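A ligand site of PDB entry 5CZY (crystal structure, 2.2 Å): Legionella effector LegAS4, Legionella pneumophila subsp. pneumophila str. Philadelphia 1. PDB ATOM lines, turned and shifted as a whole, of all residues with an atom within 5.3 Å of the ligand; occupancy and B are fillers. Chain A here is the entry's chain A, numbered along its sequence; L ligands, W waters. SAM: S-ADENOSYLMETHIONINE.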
ATOM      1  N   LEU A  63      15.123 -16.217 -17.575  1.00  0.00           N
ATOM      2  CA  LEU A  63      14.944 -15.991 -19.016  1.00  0.00           C
ATOM      3  C   LEU A  63      15.778 -16.928 -19.904  1.00  0.00           C
ATOM      4  O   LEU A  63      15.868 -16.701 -21.125  1.00  0.00           O
ATOM      5  CB  LEU A  63      15.305 -14.550 -19.381  1.00  0.00           C
ATOM      6  CG  LEU A  63      14.579 -13.475 -18.576  1.00  0.00           C
ATOM      7  CD1 LEU A  63      15.000 -12.073 -19.000  1.00  0.00           C
ATOM      8  CD2 LEU A  63      13.069 -13.650 -18.705  1.00  0.00           C
ATOM      9  N   GLY A  67      17.449 -16.997 -23.798  1.00  0.00           N
ATOM     10  CA  GLY A  67      18.777 -16.446 -23.593  1.00  0.00           C
ATOM     11  C   GLY A  67      18.822 -14.985 -23.144  1.00  0.00           C
ATOM     12  O   GLY A  67      19.772 -14.266 -23.457  1.00  0.00           O
ATOM     13  N   GLY A  68      17.811 -14.542 -22.402  1.00  0.00           N
ATOM     14  CA  GLY A  68      17.741 -13.154 -21.965  1.00  0.00           C
ATOM     15  C   GLY A  68      18.785 -12.768 -20.918  1.00  0.00           C
ATOM     16  O   GLY A  68      19.159 -13.554 -20.025  1.00  0.00           O
ATOM     17  N   ARG A  69      19.264 -11.536 -21.024  1.00  0.00           N
ATOM     18  CA  ARG A  69      20.223 -10.990 -20.106  1.00  0.00           C
ATOM     19  C   ARG A  69      19.567  -9.891 -19.276  1.00  0.00           C
ATOM     20  O   ARG A  69      18.391  -9.571 -19.493  1.00  0.00           O
ATOM     21  CB  ARG A  69      21.436 -10.455 -20.861  1.00  0.00           C
ATOM     22  CG  ARG A  69      22.239 -11.576 -21.501  1.00  0.00           C
ATOM     23  CD  ARG A  69      23.080 -11.124 -22.678  1.00  0.00           C
ATOM     24  NE  ARG A  69      23.933 -12.196 -23.181  1.00  0.00           N
ATOM     25  CZ  ARG A  69      23.550 -13.094 -24.099  1.00  0.00           C
ATOM     26  NH1 ARG A  69      22.328 -13.044 -24.622  1.00  0.00           N
ATOM     27  NH2 ARG A  69      24.413 -14.034 -24.511  1.00  0.00           N
ATOM     28  N   GLY A  70      20.320  -9.341 -18.320  1.00  0.00           N
ATOM     29  CA  GLY A  70      19.847  -8.260 -17.467  1.00  0.00           C
ATOM     30  C   GLY A  70      21.028  -7.420 -17.011  1.00  0.00           C
ATOM     31  O   GLY A  70      22.189  -7.858 -17.114  1.00  0.00           O
ATOM     32  N   TYR A  86      20.434   6.283 -22.396  1.00  0.00           N
ATOM     33  CA  TYR A  86      19.865   5.232 -23.236  1.00  0.00           C
ATOM     34  C   TYR A  86      20.180   5.550 -24.669  1.00  0.00           C
ATOM     35  O   TYR A  86      19.482   6.366 -25.303  1.00  0.00           O
ATOM     36  CB  TYR A  86      18.352   5.106 -23.008  1.00  0.00           C
ATOM     37  CG  TYR A  86      17.762   3.839 -23.621  1.00  0.00           C
ATOM     38  CD1 TYR A  86      17.209   3.860 -24.907  1.00  0.00           C
ATOM     39  CD2 TYR A  86      17.741   2.635 -22.914  1.00  0.00           C
ATOM     40  CE1 TYR A  86      16.681   2.728 -25.469  1.00  0.00           C
ATOM     41  CE2 TYR A  86      17.201   1.497 -23.472  1.00  0.00           C
ATOM     42  CZ  TYR A  86      16.678   1.552 -24.764  1.00  0.00           C
ATOM     43  OH  TYR A  86      16.131   0.431 -25.337  1.00  0.00           O
ATOM     44  N   SER A 109      10.253  -3.116 -28.837  1.00  0.00           N
ATOM     45  CA  SER A 109      10.930  -3.715 -27.677  1.00  0.00           C
ATOM     46  C   SER A 109      12.028  -2.895 -27.043  1.00  0.00           C
ATOM     47  O   SER A 109      12.176  -2.904 -25.834  1.00  0.00           O
ATOM     48  CB  SER A 109      11.588  -5.056 -28.040  1.00  0.00           C
ATOM     49  OG  SER A 109      10.647  -6.075 -27.987  1.00  0.00           O
ATOM     50  N   TYR A 110      12.846  -2.275 -27.881  1.00  0.00           N
ATOM     51  CA  TYR A 110      14.001  -1.526 -27.422  1.00  0.00           C
ATOM     52  C   TYR A 110      13.874  -0.073 -27.864  1.00  0.00           C
ATOM     53  O   TYR A 110      14.856   0.675 -27.818  1.00  0.00           O
ATOM     54  CB  TYR A 110      15.302  -2.107 -27.974  1.00  0.00           C
ATOM     55  CG  TYR A 110      15.682  -3.516 -27.497  1.00  0.00           C
ATOM     56  CD1 TYR A 110      15.011  -4.651 -27.963  1.00  0.00           C
ATOM     57  CD2 TYR A 110      16.756  -3.700 -26.620  1.00  0.00           C
ATOM     58  CE1 TYR A 110      15.383  -5.934 -27.539  1.00  0.00           C
ATOM     59  CE2 TYR A 110      17.152  -4.971 -26.203  1.00  0.00           C
ATOM     60  CZ  TYR A 110      16.458  -6.076 -26.666  1.00  0.00           C
ATOM     61  OH  TYR A 110      16.838  -7.329 -26.242  1.00  0.00           O
ATOM     62  N   ARG A 129      20.598  -0.889 -22.545  1.00  0.00           N
ATOM     63  CA  ARG A 129      19.654  -1.734 -23.309  1.00  0.00           C
ATOM     64  C   ARG A 129      19.403  -3.084 -22.628  1.00  0.00           C
ATOM     65  O   ARG A 129      18.520  -3.830 -23.092  1.00  0.00           O
ATOM     66  CB  ARG A 129      20.163  -1.980 -24.755  1.00  0.00           C
ATOM     67  CG  ARG A 129      21.312  -3.013 -24.864  1.00  0.00           C
ATOM     68  CD  ARG A 129      21.991  -2.958 -26.266  1.00  0.00           C
ATOM     69  NE  ARG A 129      21.099  -3.471 -27.311  1.00  0.00           N
ATOM     70  CZ  ARG A 129      21.027  -4.744 -27.662  1.00  0.00           C
ATOM     71  NH1 ARG A 129      21.816  -5.643 -27.065  1.00  0.00           N
ATOM     72  NH2 ARG A 129      20.175  -5.130 -28.607  1.00  0.00           N
ATOM     73  N   TYR A 130      20.155  -3.401 -21.575  1.00  0.00           N
ATOM     74  CA  TYR A 130      19.991  -4.698 -20.924  1.00  0.00           C
ATOM     75  C   TYR A 130      19.074  -4.650 -19.706  1.00  0.00           C
ATOM     76  O   TYR A 130      18.826  -5.687 -19.101  1.00  0.00           O
ATOM     77  CB  TYR A 130      21.358  -5.289 -20.533  1.00  0.00           C
ATOM     78  CG  TYR A 130      22.146  -5.718 -21.740  1.00  0.00           C
ATOM     79  CD1 TYR A 130      21.939  -6.961 -22.338  1.00  0.00           C
ATOM     80  CD2 TYR A 130      23.073  -4.857 -22.334  1.00  0.00           C
ATOM     81  CE1 TYR A 130      22.621  -7.335 -23.476  1.00  0.00           C
ATOM     82  CE2 TYR A 130      23.759  -5.219 -23.465  1.00  0.00           C
ATOM     83  CZ  TYR A 130      23.531  -6.465 -24.028  1.00  0.00           C
ATOM     84  OH  TYR A 130      24.208  -6.824 -25.159  1.00  0.00           O
ATOM     85  N   ILE A 131      18.576  -3.482 -19.338  1.00  0.00           N
ATOM     86  CA  ILE A 131      17.734  -3.387 -18.146  1.00  0.00           C
ATOM     87  C   ILE A 131      16.295  -3.879 -18.421  1.00  0.00           C
ATOM     88  O   ILE A 131      15.622  -3.375 -19.335  1.00  0.00           O
ATOM     89  CB  ILE A 131      17.671  -1.952 -17.609  1.00  0.00           C
ATOM     90  CG1 ILE A 131      19.089  -1.369 -17.460  1.00  0.00           C
ATOM     91  CG2 ILE A 131      16.949  -1.934 -16.248  1.00  0.00           C
ATOM     92  CD1 ILE A 131      19.118   0.076 -17.035  1.00  0.00           C
ATOM     93  N   ASN A 132      15.846  -4.844 -17.621  1.00  0.00           N
ATOM     94  CA  ASN A 132      14.526  -5.442 -17.800  1.00  0.00           C
ATOM     95  C   ASN A 132      13.411  -4.665 -17.095  1.00  0.00           C
ATOM     96  O   ASN A 132      13.648  -3.705 -16.350  1.00  0.00           O
ATOM     97  CB  ASN A 132      14.529  -6.899 -17.309  1.00  0.00           C
ATOM     98  CG  ASN A 132      15.347  -7.819 -18.222  1.00  0.00           C
ATOM     99  OD1 ASN A 132      15.171  -7.797 -19.443  1.00  0.00           O
ATOM    100  ND2 ASN A 132      16.268  -8.614 -17.636  1.00  0.00           N
ATOM    101  N   PHE A 133      12.195  -5.152 -17.285  1.00  0.00           N
ATOM    102  CA  PHE A 133      10.979  -4.429 -16.910  1.00  0.00           C
ATOM    103  C   PHE A 133      10.357  -4.828 -15.557  1.00  0.00           C
ATOM    104  O   PHE A 133      10.224  -6.042 -15.248  1.00  0.00           O
ATOM    105  CB  PHE A 133       9.950  -4.641 -18.041  1.00  0.00           C
ATOM    106  CG  PHE A 133       8.594  -4.072 -17.732  1.00  0.00           C
ATOM    107  CD1 PHE A 133       8.289  -2.749 -18.062  1.00  0.00           C
ATOM    108  CD2 PHE A 133       7.602  -4.871 -17.108  1.00  0.00           C
ATOM    109  CE1 PHE A 133       7.029  -2.205 -17.780  1.00  0.00           C
ATOM    110  CE2 PHE A 133       6.331  -4.330 -16.813  1.00  0.00           C
ATOM    111  CZ  PHE A 133       6.050  -2.997 -17.160  1.00  0.00           C
ATOM    112  N   TYR A 171       8.557   1.250 -18.007  1.00  0.00           N
ATOM    113  CA  TYR A 171       8.400   2.008 -19.251  1.00  0.00           C
ATOM    114  C   TYR A 171       7.218   1.466 -20.054  1.00  0.00           C
ATOM    115  O   TYR A 171       6.658   0.395 -19.726  1.00  0.00           O
ATOM    116  CB  TYR A 171       9.680   1.946 -20.107  1.00  0.00           C
ATOM    117  CG  TYR A 171      10.088   0.525 -20.451  1.00  0.00           C
ATOM    118  CD1 TYR A 171      10.913  -0.201 -19.608  1.00  0.00           C
ATOM    119  CD2 TYR A 171       9.643  -0.078 -21.622  1.00  0.00           C
ATOM    120  CE1 TYR A 171      11.286  -1.490 -19.918  1.00  0.00           C
ATOM    121  CE2 TYR A 171       9.996  -1.364 -21.941  1.00  0.00           C
ATOM    122  CZ  TYR A 171      10.826  -2.076 -21.083  1.00  0.00           C
ATOM    123  OH  TYR A 171      11.168  -3.365 -21.388  1.00  0.00           O
ATOM    124  N   GLU A 176       3.559  -5.470 -26.399  1.00  0.00           N
ATOM    125  CA  GLU A 176       4.145  -6.709 -25.880  1.00  0.00           C
ATOM    126  C   GLU A 176       3.269  -7.443 -24.889  1.00  0.00           C
ATOM    127  O   GLU A 176       3.549  -8.592 -24.584  1.00  0.00           O
ATOM    128  CB  GLU A 176       5.489  -6.421 -25.224  1.00  0.00           C
ATOM    129  CG  GLU A 176       6.493  -5.930 -26.213  1.00  0.00           C
ATOM    130  CD  GLU A 176       7.887  -6.142 -25.732  1.00  0.00           C
ATOM    131  OE1 GLU A 176       8.268  -7.327 -25.535  1.00  0.00           O
ATOM    132  OE2 GLU A 176       8.587  -5.126 -25.528  1.00  0.00           O
ATOM    133  N   TYR A 181       2.356 -11.735 -20.414  1.00  0.00           N
ATOM    134  CA  TYR A 181       3.398 -12.652 -20.901  1.00  0.00           C
ATOM    135  C   TYR A 181       4.765 -12.544 -20.239  1.00  0.00           C
ATOM    136  O   TYR A 181       5.570 -13.465 -20.382  1.00  0.00           O
ATOM    137  CB  TYR A 181       3.595 -12.481 -22.426  1.00  0.00           C
ATOM    138  CG  TYR A 181       2.368 -12.816 -23.210  1.00  0.00           C
ATOM    139  CD1 TYR A 181       1.867 -14.112 -23.228  1.00  0.00           C
ATOM    140  CD2 TYR A 181       1.691 -11.835 -23.947  1.00  0.00           C
ATOM    141  CE1 TYR A 181       0.720 -14.431 -23.943  1.00  0.00           C
ATOM    142  CE2 TYR A 181       0.533 -12.155 -24.671  1.00  0.00           C
ATOM    143  CZ  TYR A 181       0.054 -13.450 -24.671  1.00  0.00           C
ATOM    144  OH  TYR A 181      -1.089 -13.790 -25.379  1.00  0.00           O
ATOM    145  N   TYR A 182       5.052 -11.436 -19.562  1.00  0.00           N
ATOM    146  CA  TYR A 182       6.345 -11.294 -18.891  1.00  0.00           C
ATOM    147  C   TYR A 182       6.418 -12.096 -17.589  1.00  0.00           C
ATOM    148  O   TYR A 182       5.372 -12.487 -17.034  1.00  0.00           O
ATOM    149  CB  TYR A 182       6.656  -9.826 -18.586  1.00  0.00           C
ATOM    150  CG  TYR A 182       7.143  -9.043 -19.776  1.00  0.00           C
ATOM    151  CD1 TYR A 182       7.077  -9.579 -21.054  1.00  0.00           C
ATOM    152  CD2 TYR A 182       7.644  -7.768 -19.612  1.00  0.00           C
ATOM    153  CE1 TYR A 182       7.524  -8.879 -22.146  1.00  0.00           C
ATOM    154  CE2 TYR A 182       8.091  -7.030 -20.718  1.00  0.00           C
ATOM    155  CZ  TYR A 182       8.015  -7.602 -21.982  1.00  0.00           C
ATOM    156  OH  TYR A 182       8.452  -6.900 -23.073  1.00  0.00           O
ATOM    157  N   TYR A 183       7.642 -12.319 -17.113  1.00  0.00           N
ATOM    158  CA  TYR A 183       7.839 -12.730 -15.739  1.00  0.00           C
ATOM    159  C   TYR A 183       7.685 -11.523 -14.823  1.00  0.00           C
ATOM    160  O   TYR A 183       7.987 -10.362 -15.212  1.00  0.00           O
ATOM    161  CB  TYR A 183       9.227 -13.367 -15.538  1.00  0.00           C
ATOM    162  CG  TYR A 183       9.339 -14.771 -16.103  1.00  0.00           C
ATOM    163  CD1 TYR A 183       8.789 -15.856 -15.430  1.00  0.00           C
ATOM    164  CD2 TYR A 183      10.024 -15.019 -17.284  1.00  0.00           C
ATOM    165  CE1 TYR A 183       8.887 -17.169 -15.939  1.00  0.00           C
ATOM    166  CE2 TYR A 183      10.126 -16.317 -17.810  1.00  0.00           C
ATOM    167  CZ  TYR A 183       9.560 -17.384 -17.130  1.00  0.00           C
ATOM    168  OH  TYR A 183       9.646 -18.673 -17.614  1.00  0.00           O
ATOM    169  N   PHE A 184       7.211 -11.784 -13.613  1.00  0.00           N
ATOM    170  CA  PHE A 184       7.265 -10.779 -12.559  1.00  0.00           C
ATOM    171  C   PHE A 184       8.637 -10.831 -11.938  1.00  0.00           C
ATOM    172  O   PHE A 184       8.879 -11.609 -11.031  1.00  0.00           O
ATOM    173  CB  PHE A 184       6.166 -11.023 -11.514  1.00  0.00           C
ATOM    174  CG  PHE A 184       4.775 -10.792 -12.056  1.00  0.00           C
ATOM    175  CD1 PHE A 184       4.239  -9.521 -12.080  1.00  0.00           C
ATOM    176  CD2 PHE A 184       4.024 -11.842 -12.530  1.00  0.00           C
ATOM    177  CE1 PHE A 184       2.979  -9.309 -12.579  1.00  0.00           C
ATOM    178  CE2 PHE A 184       2.754 -11.633 -13.016  1.00  0.00           C
ATOM    179  CZ  PHE A 184       2.227 -10.365 -13.040  1.00  0.00           C
ATOM    180  N   LEU A 185       9.536 -10.006 -12.442  1.00  0.00           N
ATOM    181  CA  LEU A 185      10.925 -10.013 -11.978  1.00  0.00           C
ATOM    182  C   LEU A 185      11.102  -9.312 -10.623  1.00  0.00           C
ATOM    183  O   LEU A 185      10.417  -8.314 -10.340  1.00  0.00           O
ATOM    184  CB  LEU A 185      11.820  -9.349 -13.022  1.00  0.00           C
ATOM    185  CG  LEU A 185      12.034 -10.187 -14.287  1.00  0.00           C
ATOM    186  CD1 LEU A 185      12.926  -9.437 -15.254  1.00  0.00           C
ATOM    187  CD2 LEU A 185      12.635 -11.567 -13.957  1.00  0.00           C
HETATM  188  N   SAM L   1      16.541  -8.952 -21.567  1.00  0.00           N
HETATM  189  CA  SAM L   1      16.913  -8.037 -22.637  1.00  0.00           C
HETATM  190  C   SAM L   1      18.164  -8.520 -23.345  1.00  0.00           C
HETATM  191  O   SAM L   1      18.730  -9.550 -22.960  1.00  0.00           O
HETATM  192  OXT SAM L   1      18.626  -7.890 -24.319  1.00  0.00           O
HETATM  193  CB  SAM L   1      17.160  -6.612 -22.085  1.00  0.00           C
HETATM  194  CG  SAM L   1      15.872  -5.832 -21.838  1.00  0.00           C
HETATM  195  SD  SAM L   1      15.147  -5.275 -23.404  1.00  0.00           S
HETATM  196  CE  SAM L   1      15.166  -3.480 -23.109  1.00  0.00           C
HETATM  197  C5' SAM L   1      13.378  -5.631 -23.264  1.00  0.00           C
HETATM  198  C4' SAM L   1      13.093  -7.058 -23.703  1.00  0.00           C
HETATM  199  O4' SAM L   1      13.596  -7.888 -22.664  1.00  0.00           O
HETATM  200  C3' SAM L   1      11.605  -7.410 -23.848  1.00  0.00           C
HETATM  201  O3' SAM L   1      11.211  -7.370 -25.206  1.00  0.00           O
HETATM  202  C2' SAM L   1      11.508  -8.824 -23.315  1.00  0.00           C
HETATM  203  O2' SAM L   1      11.861  -9.714 -24.357  1.00  0.00           O
HETATM  204  C1' SAM L   1      12.618  -8.863 -22.290  1.00  0.00           C
HETATM  205  N9  SAM L   1      12.103  -8.552 -20.941  1.00  0.00           N
HETATM  206  C8  SAM L   1      12.294  -7.383 -20.229  1.00  0.00           C
HETATM  207  N7  SAM L   1      11.652  -7.499 -19.046  1.00  0.00           N
HETATM  208  C5  SAM L   1      11.048  -8.727 -18.988  1.00  0.00           C
HETATM  209  C6  SAM L   1      10.267  -9.379 -18.006  1.00  0.00           C
HETATM  210  N6  SAM L   1       9.972  -8.776 -16.862  1.00  0.00           N
HETATM  211  N1  SAM L   1       9.777 -10.645 -18.227  1.00  0.00           N
HETATM  212  C2  SAM L   1      10.072 -11.277 -19.414  1.00  0.00           C
HETATM  213  N3  SAM L   1      10.844 -10.621 -20.365  1.00  0.00           N
HETATM  214  C4  SAM L   1      11.326  -9.383 -20.164  1.00  0.00           C
HETATM  215  O   HOH W   1      10.364  -4.077 -23.817  1.00  0.00           O
HETATM  216  O   HOH W   2      12.127  -8.172 -27.646  1.00  0.00           O
HETATM  217  O   HOH W   3      20.503  -8.515 -26.086  1.00  0.00           O
HETATM  218  O   HOH W   4      11.326 -12.487 -22.517  1.00  0.00           O
HETATM  219  O   HOH W   5      15.401 -10.933 -23.394  1.00  0.00           O
HETATM  220  O   HOH W   6       8.593  -7.794 -13.984  1.00  0.00           O
HETATM  221  O   HOH W   7      13.182 -12.193 -26.401  1.00  0.00           O
HETATM  222  O   HOH W   8      16.252  -1.177 -20.969  1.00  0.00           O
HETATM  223  O   HOH W   9       8.830  -9.999 -25.638  1.00  0.00           O
HETATM  224  O   HOH W  10      19.955 -11.172 -24.615  1.00  0.00           O
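The backbone NH (N) of Tyr 183 sits at hydrogen-bond distance from a nitrogen (N1) of the ligand (2.9 Å).
A nitrogen (N6) of the ligand is in hydrogen-bond range of the backbone carbonyl oxygen (O) of Phe 133, at 3.2 Å.
A nitrogen (N) of the ligand sits at hydrogen-bond distance from the side-chain amide oxygen (OD1) of Asn 132, at 2.8 Å.
The backbone carbonyl oxygen of Tyr 183 is in hydrogen-bond range of a nitrogen (N6) of the ligand (3.0 Å).
The side-chain hydroxyl (OH) of Tyr 110 sits at hydrogen-bond distance from an oxygen (OXT) of the ligand (2.7 Å).
The side-chain carboxylate (OE1) of Glu 176 lies within hydrogen-bond range of an oxygen (O3') of the ligand, at 3.0 Å.
A nitrogen (N) of the ligand sits at hydrogen-bond distance from the backbone carbonyl oxygen of Arg 69, 2.8 Å away.
OG of Ser 109 lies within hydrogen-bond range of O3' of the ligand (3.1 Å).
N of Phe 133 lies within hydrogen-bond range of N7 of the ligand, 3.0 Å away.
O of the ligand is in hydrogen-bond range of N of Arg 69 (2.8 Å).
The side-chain hydroxyl of Ser 109 sits at hydrogen-bond distance from the side-chain carboxylate of Glu 176.
The guanidinium group of Arg 69 is in hydrogen-bond range of the backbone carbonyl oxygen of Gly 67 (3.1 Å).
N of Gly 68 is in hydrogen-bond range of O of Leu 63, at 3.2 Å.
The side-chain amide nitrogen of Asn 132 sits at hydrogen-bond distance from the backbone carbonyl oxygen of Arg 69 (3.0 Å).
The guanidinium group (NH1) of Arg 129 sits at hydrogen-bond distance from the side-chain hydroxyl (OH) of Tyr 130 (3.3 Å).
OE1 of Glu 176 sits at hydrogen-bond distance from OH of Tyr 182, at 2.5 Å.
O of Tyr 110 is in hydrogen-bond range of OH of Tyr 86, at 2.8 Å.
O of Arg 129 sits close to SD of the ligand, 3.7 Å away.
Leu 63 touches the ligand (CD2 to C2, 3.9 Å).
C of Gly 68 touches O of the ligand, 3.8 Å away.
Tyr 130 touches the ligand.
O of Ile 131 touches CG of the ligand, 3.5 Å away.
Tyr 171 touches the ligand (OH to C5', 3.7 Å).
CB of Tyr 182 touches N1 of the ligand, 3.2 Å away.
CD1 of Leu 185 touches N6 of the ligand (3.4 Å).
Hydrophobic or aromatic side chains that line the ligand: Leu 63, Tyr 110, Tyr 130, Phe 133, Tyr 182, Tyr 183 and Leu 185.
Within 4 Å of the ligand: Leu 63, Gly 68, Arg 69, Ser 109, Tyr 110, Arg 129, Tyr 130, Ile 131, Asn 132, Phe 133, Tyr 171, Glu 176, Tyr 182, Tyr 183 and Leu 185.
Water W10 lies within hydrogen-bond range of an oxygen (O) of the ligand, the guanidinium group of Arg 69 and the backbone carbonyl oxygen of Gly 67.
Water W3 lies within hydrogen-bond range of OXT of the ligand (2.7 Å) and NH1 of Arg 129 (3.3 Å).
Water W2 lies within hydrogen-bond range of OG of Ser 109 and O3' of the ligand.
Water W9 lies within hydrogen-bond range of the side-chain carboxylate of Glu 176 (2.7 Å) and an oxygen (O2') of the ligand (3.3 Å).
Water W6 lies within hydrogen-bond range of O of Phe 133, N of Leu 185, O of Tyr 183 and N6 of the ligand.
Water W1 lies within hydrogen-bond range of OH of Tyr 171 (2.7 Å), OE2 of Glu 176 (2.7 Å), O of Ser 109 (3.0 Å) and OH of Tyr 182 (3.5 Å).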
